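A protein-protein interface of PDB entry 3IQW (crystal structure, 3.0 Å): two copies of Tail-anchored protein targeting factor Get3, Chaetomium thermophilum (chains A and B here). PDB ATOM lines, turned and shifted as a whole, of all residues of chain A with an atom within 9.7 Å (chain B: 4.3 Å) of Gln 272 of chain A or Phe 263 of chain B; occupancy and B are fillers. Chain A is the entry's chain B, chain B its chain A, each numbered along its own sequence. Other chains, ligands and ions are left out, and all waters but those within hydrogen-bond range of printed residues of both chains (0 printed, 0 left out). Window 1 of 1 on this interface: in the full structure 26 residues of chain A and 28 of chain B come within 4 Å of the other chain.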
ATOM      1  N   LEU A 262      24.662  16.291  -7.562  1.00  0.00           N
ATOM      2  CA  LEU A 262      24.059  17.515  -7.138  1.00  0.00           C
ATOM      3  C   LEU A 262      22.597  17.179  -6.883  1.00  0.00           C
ATOM      4  O   LEU A 262      21.879  16.765  -7.792  1.00  0.00           O
ATOM      5  CB  LEU A 262      24.204  18.561  -8.241  1.00  0.00           C
ATOM      6  CG  LEU A 262      23.994  20.075  -8.053  1.00  0.00           C
ATOM      7  CD1 LEU A 262      22.518  20.491  -8.131  1.00  0.00           C
ATOM      8  CD2 LEU A 262      24.660  20.581  -6.772  1.00  0.00           C
ATOM      9  N   PHE A 263      22.168  17.310  -5.634  1.00  0.00           N
ATOM     10  CA  PHE A 263      20.758  17.215  -5.311  1.00  0.00           C
ATOM     11  C   PHE A 263      20.230  18.645  -5.107  1.00  0.00           C
ATOM     12  O   PHE A 263      20.526  19.267  -4.087  1.00  0.00           O
ATOM     13  CB  PHE A 263      20.566  16.455  -3.999  1.00  0.00           C
ATOM     14  CG  PHE A 263      21.110  15.074  -3.992  1.00  0.00           C
ATOM     15  CD1 PHE A 263      20.284  13.986  -4.202  1.00  0.00           C
ATOM     16  CD2 PHE A 263      22.437  14.857  -3.709  1.00  0.00           C
ATOM     17  CE1 PHE A 263      20.789  12.700  -4.165  1.00  0.00           C
ATOM     18  CE2 PHE A 263      22.961  13.576  -3.674  1.00  0.00           C
ATOM     19  CZ  PHE A 263      22.151  12.498  -3.904  1.00  0.00           C
ATOM     20  N   PRO A 264      19.439  19.185  -6.052  1.00  0.00           N
ATOM     21  CA  PRO A 264      18.935  20.512  -5.717  1.00  0.00           C
ATOM     22  C   PRO A 264      18.184  20.445  -4.405  1.00  0.00           C
ATOM     23  O   PRO A 264      17.684  19.374  -4.033  1.00  0.00           O
ATOM     24  CB  PRO A 264      17.939  20.815  -6.836  1.00  0.00           C
ATOM     25  CG  PRO A 264      18.227  19.848  -7.907  1.00  0.00           C
ATOM     26  CD  PRO A 264      18.840  18.644  -7.281  1.00  0.00           C
ATOM     27  N   SER A 268      13.378  24.525  -4.149  1.00  0.00           N
ATOM     28  CA  SER A 268      14.352  25.497  -4.688  1.00  0.00           C
ATOM     29  C   SER A 268      14.338  25.335  -6.187  1.00  0.00           C
ATOM     30  O   SER A 268      14.669  24.269  -6.706  1.00  0.00           O
ATOM     31  CB  SER A 268      15.763  25.209  -4.167  1.00  0.00           C
ATOM     32  OG  SER A 268      15.806  25.232  -2.756  1.00  0.00           O
ATOM     33  N   ASP A 269      13.954  26.388  -6.890  1.00  0.00           N
ATOM     34  CA  ASP A 269      13.984  26.343  -8.327  1.00  0.00           C
ATOM     35  C   ASP A 269      15.228  27.098  -8.797  1.00  0.00           C
ATOM     36  O   ASP A 269      15.406  28.278  -8.502  1.00  0.00           O
ATOM     37  CB  ASP A 269      12.752  27.030  -8.850  1.00  0.00           C
ATOM     38  CG  ASP A 269      12.789  28.494  -8.556  1.00  0.00           C
ATOM     39  OD1 ASP A 269      13.949  29.045  -8.437  1.00  0.00           O
ATOM     40  OD2 ASP A 269      11.701  29.100  -8.349  1.00  0.00           O
ATOM     41  N   CYS A 270      16.081  26.402  -9.531  1.00  0.00           N
ATOM     42  CA  CYS A 270      17.298  26.963 -10.064  1.00  0.00           C
ATOM     43  C   CYS A 270      17.428  26.472 -11.475  1.00  0.00           C
ATOM     44  O   CYS A 270      17.317  25.279 -11.722  1.00  0.00           O
ATOM     45  CB  CYS A 270      18.464  26.399  -9.289  1.00  0.00           C
ATOM     46  SG  CYS A 270      19.800  27.512  -9.122  1.00  0.00           S
ATOM     47  N   GLU A 271      17.705  27.327 -12.430  1.00  0.00           N
ATOM     48  CA  GLU A 271      17.906  26.707 -13.710  1.00  0.00           C
ATOM     49  C   GLU A 271      19.083  25.778 -13.685  1.00  0.00           C
ATOM     50  O   GLU A 271      18.948  24.585 -13.970  1.00  0.00           O
ATOM     51  CB  GLU A 271      18.083  27.729 -14.792  1.00  0.00           C
ATOM     52  CG  GLU A 271      16.676  28.262 -15.151  1.00  0.00           C
ATOM     53  CD  GLU A 271      16.722  29.671 -15.336  1.00  0.00           C
ATOM     54  OE1 GLU A 271      17.938  30.063 -15.360  1.00  0.00           O
ATOM     55  OE2 GLU A 271      15.698  30.417 -15.617  1.00  0.00           O
ATOM     56  N   GLN A 272      20.245  26.318 -13.336  1.00  0.00           N
ATOM     57  CA  GLN A 272      21.462  25.510 -13.369  1.00  0.00           C
ATOM     58  C   GLN A 272      21.264  24.307 -12.506  1.00  0.00           C
ATOM     59  O   GLN A 272      21.334  23.173 -12.963  1.00  0.00           O
ATOM     60  CB  GLN A 272      22.652  26.270 -12.813  1.00  0.00           C
ATOM     61  CG  GLN A 272      23.168  27.374 -13.687  1.00  0.00           C
ATOM     62  CD  GLN A 272      24.543  27.772 -13.253  1.00  0.00           C
ATOM     63  OE1 GLN A 272      25.464  26.977 -13.306  1.00  0.00           O
ATOM     64  NE2 GLN A 272      24.687  28.996 -12.793  1.00  0.00           N
ATOM     65  N   CYS A 273      21.047  24.562 -11.228  1.00  0.00           N
ATOM     66  CA  CYS A 273      20.780  23.482 -10.310  1.00  0.00           C
ATOM     67  C   CYS A 273      19.816  22.425 -10.873  1.00  0.00           C
ATOM     68  O   CYS A 273      20.133  21.238 -10.895  1.00  0.00           O
ATOM     69  CB  CYS A 273      20.281  24.047  -8.997  1.00  0.00           C
ATOM     70  SG  CYS A 273      21.610  24.215  -7.844  1.00  0.00           S
ATOM     71  N   THR A 274      18.650  22.852 -11.347  1.00  0.00           N
ATOM     72  CA  THR A 274      17.697  21.895 -11.888  1.00  0.00           C
ATOM     73  C   THR A 274      18.277  21.142 -13.065  1.00  0.00           C
ATOM     74  O   THR A 274      18.379  19.917 -13.031  1.00  0.00           O
ATOM     75  CB  THR A 274      16.410  22.560 -12.368  1.00  0.00           C
ATOM     76  OG1 THR A 274      15.713  23.105 -11.246  1.00  0.00           O
ATOM     77  CG2 THR A 274      15.514  21.527 -13.035  1.00  0.00           C
ATOM     78  N   ALA A 275      18.635  21.887 -14.108  1.00  0.00           N
ATOM     79  CA  ALA A 275      19.163  21.324 -15.344  1.00  0.00           C
ATOM     80  C   ALA A 275      20.319  20.373 -15.082  1.00  0.00           C
ATOM     81  O   ALA A 275      20.563  19.416 -15.821  1.00  0.00           O
ATOM     82  CB  ALA A 275      19.617  22.429 -16.245  1.00  0.00           C
ATOM     83  N   ARG A 276      21.041  20.650 -14.016  1.00  0.00           N
ATOM     84  CA  ARG A 276      22.211  19.885 -13.716  1.00  0.00           C
ATOM     85  C   ARG A 276      21.836  18.540 -13.179  1.00  0.00           C
ATOM     86  O   ARG A 276      22.422  17.523 -13.525  1.00  0.00           O
ATOM     87  CB  ARG A 276      23.004  20.599 -12.672  1.00  0.00           C
ATOM     88  CG  ARG A 276      24.462  20.393 -12.867  1.00  0.00           C
ATOM     89  CD  ARG A 276      25.111  21.685 -12.525  1.00  0.00           C
ATOM     90  NE  ARG A 276      26.498  21.625 -12.112  1.00  0.00           N
ATOM     91  CZ  ARG A 276      27.047  22.499 -11.273  1.00  0.00           C
ATOM     92  NH1 ARG A 276      26.360  23.461 -10.735  1.00  0.00           N
ATOM     93  NH2 ARG A 276      28.281  22.392 -10.907  1.00  0.00           N
ATOM     94  N   ARG A 277      20.852  18.551 -12.301  1.00  0.00           N
ATOM     95  CA  ARG A 277      20.344  17.336 -11.741  1.00  0.00           C
ATOM     96  C   ARG A 277      19.648  16.591 -12.845  1.00  0.00           C
ATOM     97  O   ARG A 277      19.586  15.377 -12.839  1.00  0.00           O
ATOM     98  CB  ARG A 277      19.374  17.656 -10.627  1.00  0.00           C
ATOM     99  CG  ARG A 277      19.406  16.642  -9.550  1.00  0.00           C
ATOM    100  CD  ARG A 277      18.156  15.835  -9.573  1.00  0.00           C
ATOM    101  NE  ARG A 277      18.280  14.647  -8.736  1.00  0.00           N
ATOM    102  CZ  ARG A 277      19.415  13.989  -8.542  1.00  0.00           C
ATOM    103  NH1 ARG A 277      20.521  14.406  -9.142  1.00  0.00           N
ATOM    104  NH2 ARG A 277      19.436  12.916  -7.755  1.00  0.00           N
ATOM    105  N   ARG A 278      19.134  17.320 -13.815  1.00  0.00           N
ATOM    106  CA  ARG A 278      18.455  16.667 -14.890  1.00  0.00           C
ATOM    107  C   ARG A 278      19.431  15.772 -15.632  1.00  0.00           C
ATOM    108  O   ARG A 278      19.134  14.600 -15.860  1.00  0.00           O
ATOM    109  CB  ARG A 278      17.832  17.693 -15.817  1.00  0.00           C
ATOM    110  CG  ARG A 278      16.491  17.273 -16.323  1.00  0.00           C
ATOM    111  CD  ARG A 278      15.953  18.288 -17.289  1.00  0.00           C
ATOM    112  NE  ARG A 278      15.086  19.303 -16.675  1.00  0.00           N
ATOM    113  CZ  ARG A 278      15.417  20.592 -16.484  1.00  0.00           C
ATOM    114  NH1 ARG A 278      16.624  21.067 -16.829  1.00  0.00           N
ATOM    115  NH2 ARG A 278      14.518  21.420 -15.943  1.00  0.00           N
ATOM    116  N   MET A 279      20.606  16.309 -15.975  1.00  0.00           N
ATOM    117  CA  MET A 279      21.574  15.583 -16.815  1.00  0.00           C
ATOM    118  C   MET A 279      22.217  14.411 -16.087  1.00  0.00           C
ATOM    119  O   MET A 279      22.330  13.315 -16.632  1.00  0.00           O
ATOM    120  CB  MET A 279      22.642  16.530 -17.373  1.00  0.00           C
ATOM    121  CG  MET A 279      23.820  16.762 -16.455  1.00  0.00           C
ATOM    122  SD  MET A 279      25.359  15.883 -16.923  1.00  0.00           S
ATOM    123  CE  MET A 279      26.271  15.790 -15.364  1.00  0.00           C
ATOM    124  N   GLN A 280      22.632  14.645 -14.851  1.00  0.00           N
ATOM    125  CA  GLN A 280      23.172  13.578 -14.023  1.00  0.00           C
ATOM    126  C   GLN A 280      22.162  12.452 -13.845  1.00  0.00           C
ATOM    127  O   GLN A 280      22.523  11.280 -13.810  1.00  0.00           O
ATOM    128  CB  GLN A 280      23.546  14.103 -12.645  1.00  0.00           C
ATOM    129  CG  GLN A 280      24.249  15.410 -12.666  1.00  0.00           C
ATOM    130  CD  GLN A 280      25.168  15.575 -11.485  1.00  0.00           C
ATOM    131  OE1 GLN A 280      24.748  15.473 -10.341  1.00  0.00           O
ATOM    132  NE2 GLN A 280      26.436  15.831 -11.757  1.00  0.00           N
ATOM    133  N   LEU B 261      34.206  27.067 -13.425  1.00  0.00           N
ATOM    134  CA  LEU B 261      33.719  28.096 -12.512  1.00  0.00           C
ATOM    135  C   LEU B 261      32.207  28.245 -12.554  1.00  0.00           C
ATOM    136  O   LEU B 261      31.616  28.438 -13.608  1.00  0.00           O
ATOM    137  CB  LEU B 261      34.369  29.429 -12.828  1.00  0.00           C
ATOM    138  CG  LEU B 261      35.865  29.377 -12.576  1.00  0.00           C
ATOM    139  CD1 LEU B 261      36.493  30.554 -13.174  1.00  0.00           C
ATOM    140  CD2 LEU B 261      36.122  29.363 -11.121  1.00  0.00           C
ATOM    141  N   LEU B 262      31.583  28.131 -11.391  1.00  0.00           N
ATOM    142  CA  LEU B 262      30.146  28.306 -11.279  1.00  0.00           C
ATOM    143  C   LEU B 262      29.905  29.805 -11.177  1.00  0.00           C
ATOM    144  O   LEU B 262      30.338  30.416 -10.228  1.00  0.00           O
ATOM    145  CB  LEU B 262      29.647  27.587 -10.022  1.00  0.00           C
ATOM    146  CG  LEU B 262      28.211  27.099  -9.825  1.00  0.00           C
ATOM    147  CD1 LEU B 262      27.352  28.180  -9.207  1.00  0.00           C
ATOM    148  CD2 LEU B 262      27.595  26.592 -11.113  1.00  0.00           C
ATOM    149  N   PHE B 263      29.270  30.417 -12.167  1.00  0.00           N
ATOM    150  CA  PHE B 263      28.822  31.799 -12.005  1.00  0.00           C
ATOM    151  C   PHE B 263      27.320  31.735 -11.781  1.00  0.00           C
ATOM    152  O   PHE B 263      26.595  31.515 -12.745  1.00  0.00           O
ATOM    153  CB  PHE B 263      28.985  32.581 -13.298  1.00  0.00           C
ATOM    154  CG  PHE B 263      30.387  32.615 -13.851  1.00  0.00           C
ATOM    155  CD1 PHE B 263      31.200  33.722 -13.631  1.00  0.00           C
ATOM    156  CD2 PHE B 263      30.892  31.581 -14.644  1.00  0.00           C
ATOM    157  CE1 PHE B 263      32.501  33.778 -14.166  1.00  0.00           C
ATOM    158  CE2 PHE B 263      32.194  31.643 -15.163  1.00  0.00           C
ATOM    159  CZ  PHE B 263      32.984  32.740 -14.918  1.00  0.00           C
ATOM    160  N   PRO B 264      26.824  31.930 -10.543  1.00  0.00           N
ATOM    161  CA  PRO B 264      25.360  31.875 -10.433  1.00  0.00           C
ATOM    162  C   PRO B 264      24.725  32.872 -11.399  1.00  0.00           C
ATOM    163  O   PRO B 264      25.345  33.885 -11.746  1.00  0.00           O
ATOM    164  CB  PRO B 264      25.083  32.330  -8.995  1.00  0.00           C
ATOM    165  CG  PRO B 264      26.387  32.292  -8.293  1.00  0.00           C
ATOM    166  CD  PRO B 264      27.469  32.408  -9.309  1.00  0.00           C
ATOM    167  N   LYS B 265      23.505  32.598 -11.841  1.00  0.00           N
ATOM    168  CA  LYS B 265      22.785  33.586 -12.627  1.00  0.00           C
ATOM    169  C   LYS B 265      22.264  34.731 -11.732  1.00  0.00           C
ATOM    170  O   LYS B 265      21.762  34.503 -10.624  1.00  0.00           O
ATOM    171  CB  LYS B 265      21.675  32.934 -13.452  1.00  0.00           C
ATOM    172  CG  LYS B 265      22.183  32.290 -14.717  1.00  0.00           C
ATOM    173  CD  LYS B 265      21.036  31.976 -15.654  1.00  0.00           C
ATOM    174  CE  LYS B 265      21.561  31.675 -17.078  1.00  0.00           C
ATOM    175  NZ  LYS B 265      20.451  31.636 -18.104  1.00  0.00           N
ATOM    176  N   ARG B 277      29.784  29.556  -5.323  1.00  0.00           N
ATOM    177  CA  ARG B 277      30.530  30.631  -5.935  1.00  0.00           C
ATOM    178  C   ARG B 277      31.324  31.331  -4.848  1.00  0.00           C
ATOM    179  O   ARG B 277      32.368  31.893  -5.080  1.00  0.00           O
ATOM    180  CB  ARG B 277      29.554  31.595  -6.586  1.00  0.00           C
ATOM    181  CG  ARG B 277      30.112  32.259  -7.783  1.00  0.00           C
ATOM    182  CD  ARG B 277      30.614  33.643  -7.452  1.00  0.00           C
ATOM    183  NE  ARG B 277      31.420  34.206  -8.530  1.00  0.00           N
ATOM    184  CZ  ARG B 277      32.221  33.496  -9.316  1.00  0.00           C
ATOM    185  NH1 ARG B 277      32.384  32.188  -9.120  1.00  0.00           N
ATOM    186  NH2 ARG B 277      32.874  34.104 -10.303  1.00  0.00           N
ATOM    187  N   LYS B 299      39.198  32.207 -17.548  1.00  0.00           N
ATOM    188  CA  LYS B 299      38.219  31.712 -16.568  1.00  0.00           C
ATOM    189  C   LYS B 299      37.028  31.040 -17.241  1.00  0.00           C
ATOM    190  O   LYS B 299      36.084  31.693 -17.590  1.00  0.00           O
ATOM    191  CB  LYS B 299      37.772  32.867 -15.646  1.00  0.00           C
ATOM    192  CG  LYS B 299      38.766  33.165 -14.549  1.00  0.00           C
ATOM    193  CD  LYS B 299      39.058  34.637 -14.382  1.00  0.00           C
ATOM    194  CE  LYS B 299      40.475  34.962 -14.822  1.00  0.00           C
ATOM    195  NZ  LYS B 299      40.878  36.427 -14.903  1.00  0.00           N
ATOM    196  N   PRO B 301      33.606  29.022 -17.652  1.00  0.00           N
ATOM    197  CA  PRO B 301      32.443  28.706 -16.838  1.00  0.00           C
ATOM    198  C   PRO B 301      32.110  27.235 -16.938  1.00  0.00           C
ATOM    199  O   PRO B 301      32.376  26.595 -17.942  1.00  0.00           O
ATOM    200  CB  PRO B 301      31.337  29.478 -17.533  1.00  0.00           C
ATOM    201  CG  PRO B 301      31.695  29.339 -18.962  1.00  0.00           C
ATOM    202  CD  PRO B 301      33.201  29.418 -19.009  1.00  0.00           C
ATOM    203  N   PHE B 324      34.828  35.419 -20.924  1.00  0.00           N
ATOM    204  CA  PHE B 324      33.461  35.263 -20.534  1.00  0.00           C
ATOM    205  C   PHE B 324      33.257  36.211 -19.376  1.00  0.00           C
ATOM    206  O   PHE B 324      34.024  36.212 -18.423  1.00  0.00           O
ATOM    207  CB  PHE B 324      33.248  33.830 -20.078  1.00  0.00           C
ATOM    208  CG  PHE B 324      31.862  33.557 -19.612  1.00  0.00           C
ATOM    209  CD1 PHE B 324      30.861  33.256 -20.521  1.00  0.00           C
ATOM    210  CD2 PHE B 324      31.540  33.622 -18.256  1.00  0.00           C
ATOM    211  CE1 PHE B 324      29.570  33.026 -20.093  1.00  0.00           C
ATOM    212  CE2 PHE B 324      30.246  33.391 -17.834  1.00  0.00           C
ATOM    213  CZ  PHE B 324      29.269  33.094 -18.759  1.00  0.00           C
ATOM    214  N   PRO B 326      29.742  37.565 -17.457  1.00  0.00           N
ATOM    215  CA  PRO B 326      28.317  37.733 -17.284  1.00  0.00           C
ATOM    216  C   PRO B 326      28.134  38.539 -16.038  1.00  0.00           C
ATOM    217  O   PRO B 326      28.797  38.262 -15.043  1.00  0.00           O
ATOM    218  CB  PRO B 326      27.842  36.300 -17.028  1.00  0.00           C
ATOM    219  CG  PRO B 326      29.056  35.611 -16.401  1.00  0.00           C
ATOM    220  CD  PRO B 326      30.271  36.493 -16.608  1.00  0.00           C
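Of the printed residues of chain B, Glu 271 of chain A touches Lys 265 (3.7 Å). Gln 272 of chain A touches just these residues of chain B: Leu 262 (3.1 Å), Phe 263 (3.2 Å), Pro 264 (3.8 Å) and Lys 265 (3.9 Å). Of the printed residues of chain B, Arg 276 of chain A touches Leu 262 (3.4 Å). Of chain A, only Gln 272 and Arg 276 come within 4 Å of Leu 262 of chain B. Of the printed residues of chain A, Lys 265 of chain B touches Glu 271 (3.7 Å) and Gln 272 (3.9 Å). The nearest residue of chain A that does not touch Phe 263 of chain B is Arg 276 of chain A (7.7 Å). The nearest printed residue of chain A that does not touch Lys 265 of chain B is Cys 270 of chain A (6.9 Å).
Positions printed for both chains: 262, 263, 264 and 277.
Among the printed residues, pairs that only touch across the chains: Gln 272 of chain A with Leu 262 of chain B (3.1 Å), Arg 276 of chain A with Leu 262 of chain B (3.4 Å), Glu 271 of chain A with Lys 265 of chain B (3.7 Å), Gln 272 of chain A with Pro 264 of chain B (3.8 Å) and Gln 272 of chain A with Lys 265 of chain B (3.9 Å).
Along chain A the printed residues that touch a printed residue of chain B span positions 271 to 276. Of the 10 printed residues of chain B, 4 touch a printed residue of chain A. Hydrophobic or aromatic side chains of chain B within 4 Å of the printed part of chain A: Leu 262.
O of Leu 262 of chain B is in hydrogen-bond range of NH1 of Arg 277 of chain B (2.9 Å).
The backbone carbonyl oxygen (O) of Phe 263 of chain B sits at hydrogen-bond distance from the side-chain amide nitrogen (NE2) of Gln 272 of chain A, 3.2 Å away.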
